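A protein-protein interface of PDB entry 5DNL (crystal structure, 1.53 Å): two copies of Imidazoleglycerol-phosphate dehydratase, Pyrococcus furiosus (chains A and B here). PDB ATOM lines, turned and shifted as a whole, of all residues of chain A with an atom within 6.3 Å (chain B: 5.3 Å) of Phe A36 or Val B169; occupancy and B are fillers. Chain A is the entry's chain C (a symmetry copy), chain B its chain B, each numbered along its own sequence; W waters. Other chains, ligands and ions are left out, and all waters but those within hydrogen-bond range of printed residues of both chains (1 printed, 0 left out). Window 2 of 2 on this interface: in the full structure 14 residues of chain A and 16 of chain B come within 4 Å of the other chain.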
ATOM      1  N   LEU A  31      -2.914  -4.915 -37.458  1.00  0.00           N
ATOM      2  CA  LEU A  31      -2.024  -6.067 -37.522  1.00  0.00           C
ATOM      3  C   LEU A  31      -1.012  -6.098 -36.385  1.00  0.00           C
ATOM      4  O   LEU A  31      -0.656  -7.176 -35.925  1.00  0.00           O
ATOM      5  CB  LEU A  31      -1.312  -6.118 -38.865  1.00  0.00           C
ATOM      6  CG  LEU A  31      -2.202  -6.362 -40.069  1.00  0.00           C
ATOM      7  CD1 LEU A  31      -1.388  -6.162 -41.334  1.00  0.00           C
ATOM      8  CD2 LEU A  31      -2.832  -7.744 -40.025  1.00  0.00           C
ATOM      9  N   THR A  32      -0.566  -4.939 -35.933  1.00  0.00           N
ATOM     10  CA  THR A  32       0.297  -4.854 -34.749  1.00  0.00           C
ATOM     11  C   THR A  32      -0.448  -5.408 -33.538  1.00  0.00           C
ATOM     12  O   THR A  32       0.090  -6.210 -32.765  1.00  0.00           O
ATOM     13  CB  THR A  32       0.765  -3.417 -34.533  1.00  0.00           C
ATOM     14  OG1 THR A  32       1.557  -2.998 -35.662  1.00  0.00           O
ATOM     15  CG2 THR A  32       1.603  -3.290 -33.273  1.00  0.00           C
ATOM     16  N   ALA A  33      -1.709  -5.021 -33.391  1.00  0.00           N
ATOM     17  CA  ALA A  33      -2.547  -5.580 -32.343  1.00  0.00           C
ATOM     18  C   ALA A  33      -2.686  -7.092 -32.495  1.00  0.00           C
ATOM     19  O   ALA A  33      -2.471  -7.836 -31.541  1.00  0.00           O
ATOM     20  CB  ALA A  33      -3.908  -4.894 -32.357  1.00  0.00           C
ATOM     21  N   PHE A  34      -3.043  -7.556 -33.689  1.00  0.00           N
ATOM     22  CA  PHE A  34      -3.204  -8.974 -33.925  1.00  0.00           C
ATOM     23  C   PHE A  34      -1.945  -9.769 -33.495  1.00  0.00           C
ATOM     24  O   PHE A  34      -2.031 -10.726 -32.741  1.00  0.00           O
ATOM     25  CB  PHE A  34      -3.506  -9.229 -35.405  1.00  0.00           C
ATOM     26  CG  PHE A  34      -3.572 -10.677 -35.731  1.00  0.00           C
ATOM     27  CD1 PHE A  34      -4.693 -11.413 -35.411  1.00  0.00           C
ATOM     28  CD2 PHE A  34      -2.457 -11.338 -36.235  1.00  0.00           C
ATOM     29  CE1 PHE A  34      -4.730 -12.783 -35.628  1.00  0.00           C
ATOM     30  CE2 PHE A  34      -2.493 -12.692 -36.458  1.00  0.00           C
ATOM     31  CZ  PHE A  34      -3.618 -13.418 -36.172  1.00  0.00           C
ATOM     32  N   ALA A  35      -0.791  -9.333 -33.977  1.00  0.00           N
ATOM     33  CA  ALA A  35       0.465 -10.038 -33.712  1.00  0.00           C
ATOM     34  C   ALA A  35       0.822 -10.023 -32.223  1.00  0.00           C
ATOM     35  O   ALA A  35       1.249 -11.033 -31.669  1.00  0.00           O
ATOM     36  CB  ALA A  35       1.567  -9.418 -34.532  1.00  0.00           C
ATOM     37  N   PHE A  36       0.597  -8.892 -31.558  1.00  0.00           N
ATOM     38  CA  PHE A  36       0.907  -8.765 -30.139  1.00  0.00           C
ATOM     39  C   PHE A  36       0.084  -9.748 -29.295  1.00  0.00           C
ATOM     40  O   PHE A  36       0.591 -10.411 -28.383  1.00  0.00           O
ATOM     41  CB  PHE A  36       0.666  -7.323 -29.689  1.00  0.00           C
ATOM     42  CG  PHE A  36       1.158  -7.031 -28.307  1.00  0.00           C
ATOM     43  CD1 PHE A  36       2.467  -6.633 -28.106  1.00  0.00           C
ATOM     44  CD2 PHE A  36       0.319  -7.142 -27.216  1.00  0.00           C
ATOM     45  CE1 PHE A  36       2.930  -6.358 -26.835  1.00  0.00           C
ATOM     46  CE2 PHE A  36       0.776  -6.859 -25.932  1.00  0.00           C
ATOM     47  CZ  PHE A  36       2.085  -6.460 -25.753  1.00  0.00           C
ATOM     48  N   TYR A  37      -1.212  -9.841 -29.595  1.00  0.00           N
ATOM     49  CA  TYR A  37      -2.086 -10.716 -28.829  1.00  0.00           C
ATOM     50  C   TYR A  37      -1.964 -12.185 -29.249  1.00  0.00           C
ATOM     51  O   TYR A  37      -2.230 -13.073 -28.440  1.00  0.00           O
ATOM     52  CB  TYR A  37      -3.538 -10.164 -28.822  1.00  0.00           C
ATOM     53  CG  TYR A  37      -3.590  -8.898 -27.983  1.00  0.00           C
ATOM     54  CD1 TYR A  37      -3.787  -8.946 -26.618  1.00  0.00           C
ATOM     55  CD2 TYR A  37      -3.327  -7.660 -28.544  1.00  0.00           C
ATOM     56  CE1 TYR A  37      -3.767  -7.783 -25.848  1.00  0.00           C
ATOM     57  CE2 TYR A  37      -3.300  -6.501 -27.787  1.00  0.00           C
ATOM     58  CZ  TYR A  37      -3.530  -6.560 -26.445  1.00  0.00           C
ATOM     59  OH  TYR A  37      -3.523  -5.401 -25.679  1.00  0.00           O
ATOM     60  N   LEU A  38      -1.554 -12.445 -30.495  1.00  0.00           N
ATOM     61  CA  LEU A  38      -1.147 -13.793 -30.923  1.00  0.00           C
ATOM     62  C   LEU A  38       0.091 -14.234 -30.136  1.00  0.00           C
ATOM     63  O   LEU A  38       0.223 -15.413 -29.845  1.00  0.00           O
ATOM     64  CB  LEU A  38      -0.897 -13.827 -32.432  1.00  0.00           C
ATOM     65  CG  LEU A  38      -0.468 -15.168 -33.031  1.00  0.00           C
ATOM     66  CD1 LEU A  38      -1.611 -16.160 -32.954  1.00  0.00           C
ATOM     67  CD2 LEU A  38       0.000 -15.027 -34.454  1.00  0.00           C
ATOM     68  N   GLY A  39       0.955 -13.280 -29.811  1.00  0.00           N
ATOM     69  CA  GLY A  39       2.190 -13.548 -29.078  1.00  0.00           C
ATOM     70  C   GLY A  39       3.348 -13.912 -29.989  1.00  0.00           C
ATOM     71  O   GLY A  39       4.270 -14.610 -29.541  1.00  0.00           O
ATOM     72  N   LYS A  40       3.324 -13.446 -31.231  1.00  0.00           N
ATOM     73  CA  LYS A  40       4.399 -13.722 -32.200  1.00  0.00           C
ATOM     74  C   LYS A  40       4.920 -12.443 -32.817  1.00  0.00           C
ATOM     75  O   LYS A  40       4.153 -11.533 -33.136  1.00  0.00           O
ATOM     76  CB  LYS A  40       3.869 -14.620 -33.327  1.00  0.00           C
ATOM     77  CG  LYS A  40       3.528 -16.025 -32.915  1.00  0.00           C
ATOM     78  CD  LYS A  40       4.719 -16.953 -33.059  1.00  0.00           C
ATOM     79  CE  LYS A  40       4.472 -18.292 -32.384  1.00  0.00           C
ATOM     80  NZ  LYS A  40       3.192 -18.930 -32.801  1.00  0.00           N
ATOM     81  N   ARG A 160      -4.028 -17.516 -30.662  1.00  0.00           N
ATOM     82  CA  ARG A 160      -2.989 -17.997 -29.737  1.00  0.00           C
ATOM     83  C   ARG A 160      -3.373 -19.351 -29.151  1.00  0.00           C
ATOM     84  O   ARG A 160      -2.540 -20.254 -29.085  1.00  0.00           O
ATOM     85  CB  ARG A 160      -2.722 -16.970 -28.634  1.00  0.00           C
ATOM     86  CG  ARG A 160      -1.623 -17.387 -27.654  1.00  0.00           C
ATOM     87  CD  ARG A 160      -1.732 -16.623 -26.350  1.00  0.00           C
ATOM     88  NE  ARG A 160      -1.311 -15.237 -26.496  1.00  0.00           N
ATOM     89  CZ  ARG A 160      -0.091 -14.757 -26.214  1.00  0.00           C
ATOM     90  NH1 ARG A 160       0.151 -13.456 -26.367  1.00  0.00           N
ATOM     91  NH2 ARG A 160       0.896 -15.541 -25.775  1.00  0.00           N
ATOM     92  N   LYS B  73       4.602  -5.759 -14.352  1.00  0.00           N
ATOM     93  CA  LYS B  73       4.076  -6.288 -15.605  1.00  0.00           C
ATOM     94  C   LYS B  73       2.996  -7.288 -15.248  1.00  0.00           C
ATOM     95  O   LYS B  73       3.245  -8.294 -14.587  1.00  0.00           O
ATOM     96  CB  LYS B  73       5.195  -6.970 -16.392  1.00  0.00           C
ATOM     97  CG  LYS B  73       6.275  -5.999 -16.841  1.00  0.00           C
ATOM     98  CD  LYS B  73       7.465  -6.740 -17.450  1.00  0.00           C
ATOM     99  CE  LYS B  73       8.601  -5.788 -17.779  1.00  0.00           C
ATOM    100  NZ  LYS B  73       9.767  -6.516 -18.346  1.00  0.00           N
ATOM    101  N   SER B 166       2.918 -10.931 -15.681  1.00  0.00           N
ATOM    102  CA  SER B 166       3.197 -11.180 -17.096  1.00  0.00           C
ATOM    103  C   SER B 166       4.686 -10.930 -17.360  1.00  0.00           C
ATOM    104  O   SER B 166       5.355 -10.218 -16.606  1.00  0.00           O
ATOM    105  CB  SER B 166       2.381 -10.207 -17.963  1.00  0.00           C
ATOM    106  OG  SER B 166       2.780 -10.262 -19.338  1.00  0.00           O
ATOM    107  N   GLU B 167       5.184 -11.489 -18.457  1.00  0.00           N
ATOM    108  CA  GLU B 167       6.553 -11.223 -18.888  1.00  0.00           C
ATOM    109  C   GLU B 167       6.750  -9.885 -19.594  1.00  0.00           C
ATOM    110  O   GLU B 167       7.881  -9.479 -19.813  1.00  0.00           O
ATOM    111  CB  GLU B 167       7.052 -12.353 -19.795  1.00  0.00           C
ATOM    112  CG  GLU B 167       7.097 -13.710 -19.110  1.00  0.00           C
ATOM    113  CD  GLU B 167       7.919 -14.734 -19.877  1.00  0.00           C
ATOM    114  OE1 GLU B 167       7.968 -14.663 -21.125  1.00  0.00           O
ATOM    115  OE2 GLU B 167       8.523 -15.613 -19.227  1.00  0.00           O
ATOM    116  N   ARG B 168       5.671  -9.186 -19.963  1.00  0.00           N
ATOM    117  CA  ARG B 168       5.804  -7.956 -20.717  1.00  0.00           C
ATOM    118  C   ARG B 168       4.763  -6.933 -20.282  1.00  0.00           C
ATOM    119  O   ARG B 168       3.763  -7.288 -19.643  1.00  0.00           O
ATOM    120  CB  ARG B 168       5.657  -8.228 -22.215  1.00  0.00           C
ATOM    121  CG  ARG B 168       4.329  -8.860 -22.576  1.00  0.00           C
ATOM    122  CD  ARG B 168       4.122  -9.133 -24.067  1.00  0.00           C
ATOM    123  NE  ARG B 168       2.754  -9.611 -24.290  1.00  0.00           N
ATOM    124  CZ  ARG B 168       2.219  -9.951 -25.478  1.00  0.00           C
ATOM    125  NH1 ARG B 168       0.942 -10.338 -25.527  1.00  0.00           N
ATOM    126  NH2 ARG B 168       2.930  -9.905 -26.584  1.00  0.00           N
ATOM    127  N   VAL B 169       5.009  -5.683 -20.654  1.00  0.00           N
ATOM    128  CA  VAL B 169       3.995  -4.629 -20.566  1.00  0.00           C
ATOM    129  C   VAL B 169       2.950  -4.971 -21.638  1.00  0.00           C
ATOM    130  O   VAL B 169       3.262  -5.046 -22.841  1.00  0.00           O
ATOM    131  CB  VAL B 169       4.587  -3.229 -20.810  1.00  0.00           C
ATOM    132  CG1 VAL B 169       3.492  -2.165 -20.818  1.00  0.00           C
ATOM    133  CG2 VAL B 169       5.626  -2.903 -19.727  1.00  0.00           C
ATOM    134  N   GLU B 170       1.701  -5.192 -21.218  1.00  0.00           N
ATOM    135  CA  GLU B 170       0.701  -5.767 -22.112  1.00  0.00           C
ATOM    136  C   GLU B 170      -0.041  -4.681 -22.902  1.00  0.00           C
ATOM    137  O   GLU B 170      -1.249  -4.527 -22.774  1.00  0.00           O
ATOM    138  CB  GLU B 170      -0.267  -6.639 -21.303  1.00  0.00           C
ATOM    139  CG  GLU B 170       0.336  -7.943 -20.819  1.00  0.00           C
ATOM    140  CD  GLU B 170       0.537  -8.975 -21.917  1.00  0.00           C
ATOM    141  OE1 GLU B 170      -0.098  -8.886 -22.999  1.00  0.00           O
ATOM    142  OE2 GLU B 170       1.287  -9.942 -21.654  1.00  0.00           O
ATOM    143  N   SER B 171       0.684  -3.944 -23.727  1.00  0.00           N
ATOM    144  CA  SER B 171       0.109  -2.937 -24.606  1.00  0.00           C
ATOM    145  C   SER B 171       1.027  -2.697 -25.790  1.00  0.00           C
ATOM    146  O   SER B 171       2.228  -2.502 -25.624  1.00  0.00           O
ATOM    147  CB  SER B 171      -0.095  -1.610 -23.883  1.00  0.00           C
ATOM    148  OG  SER B 171      -0.548  -0.623 -24.798  1.00  0.00           O
ATOM    149  N   THR B 172       0.442  -2.626 -26.976  1.00  0.00           N
ATOM    150  CA  THR B 172       1.199  -2.316 -28.178  1.00  0.00           C
ATOM    151  C   THR B 172       1.766  -0.886 -28.156  1.00  0.00           C
ATOM    152  O   THR B 172       2.712  -0.589 -28.894  1.00  0.00           O
ATOM    153  CB  THR B 172       0.360  -2.477 -29.465  1.00  0.00           C
ATOM    154  OG1 THR B 172      -0.812  -1.642 -29.396  1.00  0.00           O
ATOM    155  CG2 THR B 172      -0.049  -3.911 -29.668  1.00  0.00           C
ATOM    156  N   GLY B 174       3.161   0.457 -25.604  1.00  0.00           N
ATOM    157  CA  GLY B 174       4.389   0.354 -24.812  1.00  0.00           C
ATOM    158  C   GLY B 174       4.242   0.845 -23.393  1.00  0.00           C
ATOM    159  O   GLY B 174       5.189   0.763 -22.610  1.00  0.00           O
ATOM    160  N   VAL B 175       3.069   1.366 -23.048  1.00  0.00           N
ATOM    161  CA  VAL B 175       2.824   1.883 -21.711  1.00  0.00           C
ATOM    162  C   VAL B 175       1.337   1.759 -21.421  1.00  0.00           C
ATOM    163  O   VAL B 175       0.508   1.685 -22.358  1.00  0.00           O
ATOM    164  CB  VAL B 175       3.373   3.321 -21.562  1.00  0.00           C
ATOM    165  CG1 VAL B 175       2.753   4.252 -22.578  1.00  0.00           C
ATOM    166  CG2 VAL B 175       3.177   3.854 -20.146  1.00  0.00           C
ATOM    167  N   LEU B 176       1.018   1.653 -20.138  1.00  0.00           N
ATOM    168  CA  LEU B 176      -0.359   1.740 -19.704  1.00  0.00           C
ATOM    169  C   LEU B 176      -0.526   3.116 -19.020  1.00  0.00           C
ATOM    170  O   LEU B 176      -1.379   3.959 -19.339  1.00  0.00           O
ATOM    171  CB  LEU B 176      -0.713   0.503 -18.862  1.00  0.00           C
ATOM    172  CG  LEU B 176      -0.820  -0.793 -19.712  1.00  0.00           C
ATOM    173  CD1 LEU B 176      -0.752  -2.093 -18.914  1.00  0.00           C
ATOM    174  CD2 LEU B 176      -2.096  -0.798 -20.557  1.00  0.00           C
ATOM    175  OXT LEU B 176       0.263   3.503 -18.170  1.00  0.00           O
HETATM  176  O   HOH W   1      -2.499  -3.282 -26.901  1.00  0.00           O
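Val B169 touches just one residue of chain A: Phe A36 (3.4 Å). Printed residues of chain A within 4 Å of Thr B172: Thr A32 (3.9 Å) and Phe A36 (3.5 Å). Printed residues of chain B within 4 Å of Thr A32: Thr B172. Of the printed residues of chain A, Ser B171 touches Phe A36 (3.5 Å). Of the printed residues of chain B, Arg A160 touches Arg B168 (3.3 Å). Of the printed residues of chain B, Tyr A37 touches Glu B170.
No position is printed for both chains. Of the 8 pairs that touch across the chains among the printed residues, none has its exchanged pair printed and touching as well.
The backbone carbonyl oxygen (O) of Arg B168 is in hydrogen-bond range of the side-chain hydroxyl (OG) of Ser B166 (3.1 Å). OG of Ser B166 sits at hydrogen-bond distance from OE2 of Glu B170 (2.8 Å). The guanidinium group (NE) of Arg B168 is in salt-bridge range of the side-chain carboxylate (OE2) of Glu B170, at 3.0 Å. O of Tyr A37 lies within hydrogen-bond range of NE of Arg A160, 3.1 Å away.
Among the printed residues, merely in contact across the chains: Phe A36 with Val B169 (3.4 Å), Phe A36 with Thr B172 (3.5 Å), Phe A36 with Ser B171 (3.5 Å), Phe A36 with Glu B170 (3.7 Å), Tyr A37 with Glu B170 (3.8 Å) and Thr A32 with Thr B172 (3.9 Å).
Printed residues of chain B that touch a printed residue of chain A: Arg B168, Val B169, Glu B170, Ser B171 and Thr B172. Among the printed residues, no Asp or Glu carboxylate lies within 4 Å of a Lys or Arg side-chain nitrogen of the other chain.
The guanidinium group of Arg B168 lies within hydrogen-bond range of the backbone carbonyl oxygen of Phe A36, 2.9 Å away. NH1 of Arg A160 sits close to NH1 of Arg B168 (3.3 Å).
Water W1 bridges the side-chain hydroxyl of Tyr A37 (2.7 Å) and the backbone NH of Thr B172 (3.0 Å).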
